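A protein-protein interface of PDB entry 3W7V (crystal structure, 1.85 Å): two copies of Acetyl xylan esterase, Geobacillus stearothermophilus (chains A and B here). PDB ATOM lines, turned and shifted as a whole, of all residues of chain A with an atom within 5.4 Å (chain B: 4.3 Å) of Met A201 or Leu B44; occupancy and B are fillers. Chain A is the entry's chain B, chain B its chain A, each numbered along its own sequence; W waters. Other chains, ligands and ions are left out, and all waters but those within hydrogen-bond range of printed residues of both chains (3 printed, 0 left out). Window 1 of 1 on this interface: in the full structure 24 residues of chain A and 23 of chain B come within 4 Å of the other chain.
The guanidinium group of Arg A205 lies within hydrogen-bond range of the backbone carbonyl oxygen of Trp B215.
O of Leu B208 sits at hydrogen-bond distance from N of Phe B213 (3.0 Å).
The side-chain hydroxyl (OG) of Ser A196 lies close to the backbone NH (N) of Ala A198 (3.2 Å).
Met B201 touches Tyr A40 (CE to CB, 3.7 Å).
Ala A198 touches Gly B43.
Ala A198 touches Gln B46 (CB to OE1, 3.2 Å).
Met A201 touches Tyr B40 (CE to CB, 3.6 Å).
CB of Met A201 touches O of Gly B43 (3.9 Å).
Leu B44 touches Met A201 (CG to SD, 3.8 Å).
Met A201 touches Met B201.
Ala B47 touches Ile A202.
Val B48 touches Arg A205.
CE3 of Trp A215 touches CE3 of Trp B215 (3.4 Å).
Val A197 touches none of the printed residues of chain B.
Of chain B, only Tyr B40, Gly B43, Leu B44 and Met B201 come within 4 Å of Met A201.
Of the printed residues of chain A, Tyr B40 touches Tyr A40 and Met A201.
Leu B44 touches one residue of chain A.
Leu B45 touches none of the printed residues of chain A.
Of the printed residues of chain A, Ala B47 touches Ile A202.
Printed residues of chain A within 4 Å of Met B201: Tyr A40, Leu A44 and Met A201.
The nearest printed residue of chain B that does not touch Met A201 is Ala B47 (4.3 Å).
The nearest residue of chain A that does not touch Leu B44 is Trp A215 (4.3 Å).
Hydrophobic or aromatic side chains of chain B that line the printed part of chain A: Tyr B40, Leu B44, Ala B47, Val B48, Met B201, Phe B213 and Trp B215.
Among the printed residues, no Asp or Glu carboxylate lies within 4 Å of a Lys or Arg side-chain nitrogen of the other chain.
Tyr B40 touches its own counterpart, Tyr A40.
Tyr A40 touches Met B201, and with the chains exchanged Met A201 touches Tyr B40.
Leu A44 touches Met B201, and with the chains exchanged Met A201 touches Leu B44.
Met B201 touches its own counterpart, Met A201.
Positions printed for both chains: 40, 44, 201 and 215.
Of the 14 pairs that touch across the chains among the printed residues, 7 have their exchanged pair printed and touching as well.
Water W3 lies within hydrogen-bond range of the side-chain amide oxygen of Gln B46 and the side-chain hydroxyl of Ser A196.
Water W2 bridges O of Phe B213 (2.6 Å) and NE1 of Trp A215 (2.9 Å).
Water W1 bridges O of Ala B47 (2.9 Å) and NH1 of Arg A205 (3.2 Å).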
ATOM      1  N   TYR A  40      10.324  11.771 -11.988  1.00  0.00           N
ATOM      2  CA  TYR A  40      10.473  13.135 -11.431  1.00  0.00           C
ATOM      3  C   TYR A  40      11.609  13.853 -12.126  1.00  0.00           C
ATOM      4  O   TYR A  40      11.502  15.083 -12.432  1.00  0.00           O
ATOM      5  CB  TYR A  40      10.707  13.123  -9.955  1.00  0.00           C
ATOM      6  CG  TYR A  40       9.652  12.481  -9.081  1.00  0.00           C
ATOM      7  CD1 TYR A  40       8.383  12.209  -9.533  1.00  0.00           C
ATOM      8  CD2 TYR A  40       9.892  12.284  -7.768  1.00  0.00           C
ATOM      9  CE1 TYR A  40       7.395  11.655  -8.736  1.00  0.00           C
ATOM     10  CE2 TYR A  40       8.944  11.743  -6.949  1.00  0.00           C
ATOM     11  CZ  TYR A  40       7.692  11.370  -7.438  1.00  0.00           C
ATOM     12  OH  TYR A  40       6.729  10.850  -6.619  1.00  0.00           O
ATOM     13  N   LEU A  44      11.068  17.356 -14.140  1.00  0.00           N
ATOM     14  CA  LEU A  44      11.768  18.573 -13.835  1.00  0.00           C
ATOM     15  C   LEU A  44      12.588  19.012 -15.062  1.00  0.00           C
ATOM     16  O   LEU A  44      12.693  20.166 -15.305  1.00  0.00           O
ATOM     17  CB  LEU A  44      12.701  18.389 -12.628  1.00  0.00           C
ATOM     18  CG  LEU A  44      11.882  18.473 -11.309  1.00  0.00           C
ATOM     19  CD1 LEU A  44      12.632  17.869 -10.140  1.00  0.00           C
ATOM     20  CD2 LEU A  44      11.482  19.902 -11.009  1.00  0.00           C
ATOM     21  N   SER A 196       8.741   7.076   0.292  1.00  0.00           N
ATOM     22  CA  SER A 196       7.640   7.929  -0.094  1.00  0.00           C
ATOM     23  C   SER A 196       8.060   8.815  -1.273  1.00  0.00           C
ATOM     24  O   SER A 196       9.234   8.800  -1.681  1.00  0.00           O
ATOM     25  CB  SER A 196       7.357   8.905   1.083  1.00  0.00           C
ATOM     26  OG  SER A 196       8.488   9.670   1.384  1.00  0.00           O
ATOM     27  N   VAL A 197       7.135   9.613  -1.770  1.00  0.00           N
ATOM     28  CA  VAL A 197       7.429  10.634  -2.754  1.00  0.00           C
ATOM     29  C   VAL A 197       8.657  11.436  -2.290  1.00  0.00           C
ATOM     30  O   VAL A 197       9.533  11.749  -3.070  1.00  0.00           O
ATOM     31  CB  VAL A 197       6.204  11.526  -2.950  1.00  0.00           C
ATOM     32  CG1 VAL A 197       6.557  12.728  -3.787  1.00  0.00           C
ATOM     33  CG2 VAL A 197       5.069  10.735  -3.582  1.00  0.00           C
ATOM     34  N   ALA A 198       8.731  11.758  -1.016  1.00  0.00           N
ATOM     35  CA  ALA A 198       9.844  12.523  -0.508  1.00  0.00           C
ATOM     36  C   ALA A 198      11.182  11.835  -0.757  1.00  0.00           C
ATOM     37  O   ALA A 198      12.114  12.477  -1.143  1.00  0.00           O
ATOM     38  CB  ALA A 198       9.663  12.815   0.973  1.00  0.00           C
ATOM     39  N   GLY A 199      11.247  10.537  -0.532  1.00  0.00           N
ATOM     40  CA  GLY A 199      12.498   9.800  -0.816  1.00  0.00           C
ATOM     41  C   GLY A 199      12.875   9.852  -2.267  1.00  0.00           C
ATOM     42  O   GLY A 199      14.036   9.976  -2.662  1.00  0.00           O
ATOM     43  N   HIS A 200      11.867   9.678  -3.121  1.00  0.00           N
ATOM     44  CA  HIS A 200      12.079   9.799  -4.542  1.00  0.00           C
ATOM     45  C   HIS A 200      12.509  11.173  -4.955  1.00  0.00           C
ATOM     46  O   HIS A 200      13.271  11.300  -5.888  1.00  0.00           O
ATOM     47  CB  HIS A 200      10.866   9.177  -5.341  1.00  0.00           C
ATOM     48  CG  HIS A 200      10.966   7.708  -5.431  1.00  0.00           C
ATOM     49  ND1 HIS A 200      10.281   6.808  -4.604  1.00  0.00           N
ATOM     50  CD2 HIS A 200      11.741   6.967  -6.243  1.00  0.00           C
ATOM     51  CE1 HIS A 200      10.671   5.582  -4.908  1.00  0.00           C
ATOM     52  NE2 HIS A 200      11.545   5.660  -5.897  1.00  0.00           N
ATOM     53  N   MET A 201      12.040  12.238  -4.283  1.00  0.00           N
ATOM     54  CA  MET A 201      12.493  13.576  -4.566  1.00  0.00           C
ATOM     55  C   MET A 201      13.938  13.746  -4.089  1.00  0.00           C
ATOM     56  O   MET A 201      14.693  14.475  -4.719  1.00  0.00           O
ATOM     57  CB  MET A 201      11.596  14.664  -3.906  1.00  0.00           C
ATOM     58  CG  MET A 201      10.257  14.820  -4.558  1.00  0.00           C
ATOM     59  SD  MET A 201      10.499  15.556  -6.185  1.00  0.00           S
ATOM     60  CE  MET A 201       8.740  15.727  -6.459  1.00  0.00           C
ATOM     61  N   ILE A 202      14.297  13.101  -2.976  1.00  0.00           N
ATOM     62  CA  ILE A 202      15.703  13.136  -2.425  1.00  0.00           C
ATOM     63  C   ILE A 202      16.590  12.609  -3.566  1.00  0.00           C
ATOM     64  O   ILE A 202      17.636  13.181  -3.907  1.00  0.00           O
ATOM     65  CB  ILE A 202      15.833  12.332  -1.149  1.00  0.00           C
ATOM     66  CG1 ILE A 202      15.152  13.117  -0.014  1.00  0.00           C
ATOM     67  CG2 ILE A 202      17.323  12.079  -0.768  1.00  0.00           C
ATOM     68  CD1 ILE A 202      14.945  12.362   1.267  1.00  0.00           C
ATOM     69  N   LEU A 203      16.173  11.505  -4.138  1.00  0.00           N
ATOM     70  CA  LEU A 203      16.963  10.866  -5.181  1.00  0.00           C
ATOM     71  C   LEU A 203      17.007  11.694  -6.438  1.00  0.00           C
ATOM     72  O   LEU A 203      18.034  11.857  -7.090  1.00  0.00           O
ATOM     73  CB  LEU A 203      16.342   9.533  -5.526  1.00  0.00           C
ATOM     74  CG  LEU A 203      16.532   8.488  -4.411  1.00  0.00           C
ATOM     75  CD1 LEU A 203      15.647   7.258  -4.602  1.00  0.00           C
ATOM     76  CD2 LEU A 203      17.945   8.008  -4.373  1.00  0.00           C
ATOM     77  N   ALA A 204      15.843  12.154  -6.867  1.00  0.00           N
ATOM     78  CA  ALA A 204      15.772  12.923  -8.111  1.00  0.00           C
ATOM     79  C   ALA A 204      16.645  14.189  -7.992  1.00  0.00           C
ATOM     80  O   ALA A 204      17.409  14.524  -8.903  1.00  0.00           O
ATOM     81  CB  ALA A 204      14.340  13.322  -8.422  1.00  0.00           C
ATOM     82  N   ARG A 205      16.559  14.861  -6.868  1.00  0.00           N
ATOM     83  CA  ARG A 205      17.363  16.057  -6.636  1.00  0.00           C
ATOM     84  C   ARG A 205      18.862  15.770  -6.653  1.00  0.00           C
ATOM     85  O   ARG A 205      19.663  16.526  -7.233  1.00  0.00           O
ATOM     86  CB  ARG A 205      16.899  16.729  -5.325  1.00  0.00           C
ATOM     87  CG  ARG A 205      17.789  17.891  -4.853  1.00  0.00           C
ATOM     88  CD  ARG A 205      17.023  18.730  -3.864  1.00  0.00           C
ATOM     89  NE  ARG A 205      17.805  19.780  -3.215  1.00  0.00           N
ATOM     90  CZ  ARG A 205      18.509  19.607  -2.112  1.00  0.00           C
ATOM     91  NH1 ARG A 205      18.679  18.380  -1.582  1.00  0.00           N
ATOM     92  NH2 ARG A 205      19.096  20.683  -1.544  1.00  0.00           N
ATOM     93  N   ALA A 206      19.226  14.696  -5.972  1.00  0.00           N
ATOM     94  CA  ALA A 206      20.625  14.327  -5.921  1.00  0.00           C
ATOM     95  C   ALA A 206      21.177  14.038  -7.342  1.00  0.00           C
ATOM     96  O   ALA A 206      22.318  14.449  -7.717  1.00  0.00           O
ATOM     97  CB  ALA A 206      20.779  13.127  -5.011  1.00  0.00           C
ATOM     98  N   TRP A 215      17.640  24.987 -10.837  1.00  0.00           N
ATOM     99  CA  TRP A 215      16.233  25.116 -10.548  1.00  0.00           C
ATOM    100  C   TRP A 215      15.641  26.389 -11.176  1.00  0.00           C
ATOM    101  O   TRP A 215      14.528  26.354 -11.691  1.00  0.00           O
ATOM    102  CB  TRP A 215      16.092  25.194  -9.092  1.00  0.00           C
ATOM    103  CG  TRP A 215      14.750  25.468  -8.512  1.00  0.00           C
ATOM    104  CD1 TRP A 215      14.389  26.609  -7.880  1.00  0.00           C
ATOM    105  CD2 TRP A 215      13.639  24.563  -8.361  1.00  0.00           C
ATOM    106  NE1 TRP A 215      13.124  26.501  -7.351  1.00  0.00           N
ATOM    107  CE2 TRP A 215      12.638  25.257  -7.639  1.00  0.00           C
ATOM    108  CE3 TRP A 215      13.390  23.228  -8.745  1.00  0.00           C
ATOM    109  CZ2 TRP A 215      11.434  24.680  -7.304  1.00  0.00           C
ATOM    110  CZ3 TRP A 215      12.218  22.647  -8.387  1.00  0.00           C
ATOM    111  CH2 TRP A 215      11.234  23.364  -7.658  1.00  0.00           C
ATOM    112  N   TYR B  40       4.138  16.592  -4.788  1.00  0.00           N
ATOM    113  CA  TYR B  40       5.451  16.980  -5.193  1.00  0.00           C
ATOM    114  C   TYR B  40       5.956  18.116  -4.286  1.00  0.00           C
ATOM    115  O   TYR B  40       7.150  18.139  -3.915  1.00  0.00           O
ATOM    116  CB  TYR B  40       5.518  17.414  -6.667  1.00  0.00           C
ATOM    117  CG  TYR B  40       5.154  16.353  -7.699  1.00  0.00           C
ATOM    118  CD1 TYR B  40       5.054  15.004  -7.365  1.00  0.00           C
ATOM    119  CD2 TYR B  40       4.988  16.707  -8.989  1.00  0.00           C
ATOM    120  CE1 TYR B  40       4.724  14.055  -8.322  1.00  0.00           C
ATOM    121  CE2 TYR B  40       4.649  15.777  -9.937  1.00  0.00           C
ATOM    122  CZ  TYR B  40       4.531  14.449  -9.583  1.00  0.00           C
ATOM    123  OH  TYR B  40       4.195  13.575 -10.551  1.00  0.00           O
ATOM    124  N   VAL B  41       5.080  19.091  -3.999  1.00  0.00           N
ATOM    125  CA  VAL B  41       5.450  20.185  -3.113  1.00  0.00           C
ATOM    126  C   VAL B  41       5.840  19.630  -1.745  1.00  0.00           C
ATOM    127  O   VAL B  41       6.895  19.943  -1.177  1.00  0.00           O
ATOM    128  CB  VAL B  41       4.262  21.158  -2.964  1.00  0.00           C
ATOM    129  CG1 VAL B  41       4.472  22.104  -1.753  1.00  0.00           C
ATOM    130  CG2 VAL B  41       4.085  21.939  -4.258  1.00  0.00           C
ATOM    131  N   VAL B  42       5.053  18.713  -1.244  1.00  0.00           N
ATOM    132  CA  VAL B  42       5.298  18.128   0.095  1.00  0.00           C
ATOM    133  C   VAL B  42       6.595  17.302   0.084  1.00  0.00           C
ATOM    134  O   VAL B  42       7.427  17.436   0.989  1.00  0.00           O
ATOM    135  CB  VAL B  42       4.101  17.293   0.577  1.00  0.00           C
ATOM    136  CG1 VAL B  42       4.384  16.679   1.935  1.00  0.00           C
ATOM    137  CG2 VAL B  42       2.886  18.176   0.756  1.00  0.00           C
ATOM    138  N   GLY B  43       6.823  16.541  -0.982  1.00  0.00           N
ATOM    139  CA  GLY B  43       8.078  15.841  -1.197  1.00  0.00           C
ATOM    140  C   GLY B  43       9.304  16.686  -1.229  1.00  0.00           C
ATOM    141  O   GLY B  43      10.326  16.365  -0.607  1.00  0.00           O
ATOM    142  N   LEU B  44       9.275  17.764  -1.990  1.00  0.00           N
ATOM    143  CA  LEU B  44      10.384  18.639  -2.071  1.00  0.00           C
ATOM    144  C   LEU B  44      10.624  19.392  -0.786  1.00  0.00           C
ATOM    145  O   LEU B  44      11.793  19.559  -0.375  1.00  0.00           O
ATOM    146  CB  LEU B  44      10.256  19.604  -3.243  1.00  0.00           C
ATOM    147  CG  LEU B  44      10.575  18.982  -4.622  1.00  0.00           C
ATOM    148  CD1 LEU B  44       9.989  19.763  -5.772  1.00  0.00           C
ATOM    149  CD2 LEU B  44      12.085  18.828  -4.751  1.00  0.00           C
ATOM    150  N   LEU B  45       9.574  19.819  -0.115  1.00  0.00           N
ATOM    151  CA  LEU B  45       9.770  20.438   1.213  1.00  0.00           C
ATOM    152  C   LEU B  45      10.434  19.499   2.224  1.00  0.00           C
ATOM    153  O   LEU B  45      11.270  19.946   3.027  1.00  0.00           O
ATOM    154  CB  LEU B  45       8.423  20.905   1.746  1.00  0.00           C
ATOM    155  CG  LEU B  45       7.908  22.159   1.052  1.00  0.00           C
ATOM    156  CD1 LEU B  45       6.566  22.519   1.590  1.00  0.00           C
ATOM    157  CD2 LEU B  45       8.870  23.308   1.290  1.00  0.00           C
ATOM    158  N   GLN B  46      10.054  18.225   2.188  1.00  0.00           N
ATOM    159  CA  GLN B  46      10.621  17.268   3.084  1.00  0.00           C
ATOM    160  C   GLN B  46      12.060  16.941   2.716  1.00  0.00           C
ATOM    161  O   GLN B  46      12.909  16.780   3.616  1.00  0.00           O
ATOM    162  CB  GLN B  46       9.763  16.049   3.196  1.00  0.00           C
ATOM    163  CG  GLN B  46      10.234  15.156   4.311  1.00  0.00           C
ATOM    164  CD  GLN B  46       9.171  14.170   4.770  1.00  0.00           C
ATOM    165  OE1 GLN B  46       8.781  13.246   4.041  1.00  0.00           O
ATOM    166  NE2 GLN B  46       8.687  14.371   5.995  1.00  0.00           N
ATOM    167  N   ALA B  47      12.348  16.874   1.418  1.00  0.00           N
ATOM    168  CA  ALA B  47      13.685  16.602   0.969  1.00  0.00           C
ATOM    169  C   ALA B  47      14.655  17.714   1.292  1.00  0.00           C
ATOM    170  O   ALA B  47      15.871  17.451   1.508  1.00  0.00           O
ATOM    171  CB  ALA B  47      13.728  16.385  -0.544  1.00  0.00           C
ATOM    172  N   VAL B  48      14.179  18.976   1.217  1.00  0.00           N
ATOM    173  CA  VAL B  48      15.071  20.121   1.394  1.00  0.00           C
ATOM    174  C   VAL B  48      14.938  20.851   2.773  1.00  0.00           C
ATOM    175  O   VAL B  48      15.937  21.406   3.308  1.00  0.00           O
ATOM    176  CB  VAL B  48      14.907  21.086   0.200  1.00  0.00           C
ATOM    177  CG1 VAL B  48      15.870  22.295   0.292  1.00  0.00           C
ATOM    178  CG2 VAL B  48      15.056  20.306  -1.098  1.00  0.00           C
ATOM    179  N   MET B 201       5.024  19.223 -12.140  1.00  0.00           N
ATOM    180  CA  MET B 201       6.268  19.851 -11.679  1.00  0.00           C
ATOM    181  C   MET B 201       6.284  21.352 -11.969  1.00  0.00           C
ATOM    182  O   MET B 201       6.768  22.147 -11.163  1.00  0.00           O
ATOM    183  CB  MET B 201       7.474  19.200 -12.371  1.00  0.00           C
ATOM    184  CG  MET B 201       7.792  17.824 -11.840  1.00  0.00           C
ATOM    185  SD  MET B 201       8.325  17.882 -10.116  1.00  0.00           S
ATOM    186  CE  MET B 201       8.558  16.120  -9.995  1.00  0.00           C
ATOM    187  N   LEU B 208       6.311  26.596  -5.040  1.00  0.00           N
ATOM    188  CA  LEU B 208       7.508  26.692  -4.194  1.00  0.00           C
ATOM    189  C   LEU B 208       8.241  28.011  -4.321  1.00  0.00           C
ATOM    190  O   LEU B 208       8.703  28.562  -3.338  1.00  0.00           O
ATOM    191  CB  LEU B 208       8.391  25.497  -4.579  1.00  0.00           C
ATOM    192  CG  LEU B 208       7.871  24.194  -4.025  1.00  0.00           C
ATOM    193  CD1 LEU B 208       8.626  23.000  -4.550  1.00  0.00           C
ATOM    194  CD2 LEU B 208       7.956  24.130  -2.509  1.00  0.00           C
ATOM    195  N   PHE B 213      10.933  28.880  -1.320  1.00  0.00           N
ATOM    196  CA  PHE B 213      11.759  27.645  -1.420  1.00  0.00           C
ATOM    197  C   PHE B 213      13.041  27.922  -2.103  1.00  0.00           C
ATOM    198  O   PHE B 213      13.101  28.586  -3.171  1.00  0.00           O
ATOM    199  CB  PHE B 213      10.938  26.536  -2.144  1.00  0.00           C
ATOM    200  CG  PHE B 213      11.693  25.245  -2.481  1.00  0.00           C
ATOM    201  CD1 PHE B 213      11.670  24.175  -1.660  1.00  0.00           C
ATOM    202  CD2 PHE B 213      12.305  25.128  -3.695  1.00  0.00           C
ATOM    203  CE1 PHE B 213      12.266  22.988  -2.028  1.00  0.00           C
ATOM    204  CE2 PHE B 213      12.936  23.954  -4.104  1.00  0.00           C
ATOM    205  CZ  PHE B 213      12.912  22.878  -3.216  1.00  0.00           C
ATOM    206  N   TRP B 215      16.130  25.608  -3.769  1.00  0.00           N
ATOM    207  CA  TRP B 215      16.561  24.277  -4.236  1.00  0.00           C
ATOM    208  C   TRP B 215      17.806  23.774  -3.507  1.00  0.00           C
ATOM    209  O   TRP B 215      17.849  22.649  -3.024  1.00  0.00           O
ATOM    210  CB  TRP B 215      16.773  24.346  -5.725  1.00  0.00           C
ATOM    211  CG  TRP B 215      17.313  23.090  -6.384  1.00  0.00           C
ATOM    212  CD1 TRP B 215      18.548  22.924  -6.906  1.00  0.00           C
ATOM    213  CD2 TRP B 215      16.583  21.886  -6.698  1.00  0.00           C
ATOM    214  NE1 TRP B 215      18.669  21.697  -7.510  1.00  0.00           N
ATOM    215  CE2 TRP B 215      17.492  21.013  -7.369  1.00  0.00           C
ATOM    216  CE3 TRP B 215      15.260  21.488  -6.528  1.00  0.00           C
ATOM    217  CZ2 TRP B 215      17.107  19.788  -7.884  1.00  0.00           C
ATOM    218  CZ3 TRP B 215      14.869  20.254  -7.021  1.00  0.00           C
ATOM    219  CH2 TRP B 215      15.815  19.411  -7.689  1.00  0.00           C
HETATM  220  O   HOH W   1      17.742  15.777   0.072  1.00  0.00           O
HETATM  221  O   HOH W   2      12.683  28.832  -5.691  1.00  0.00           O
HETATM  222  O   HOH W   3       8.136  10.867   3.717  1.00  0.00           O
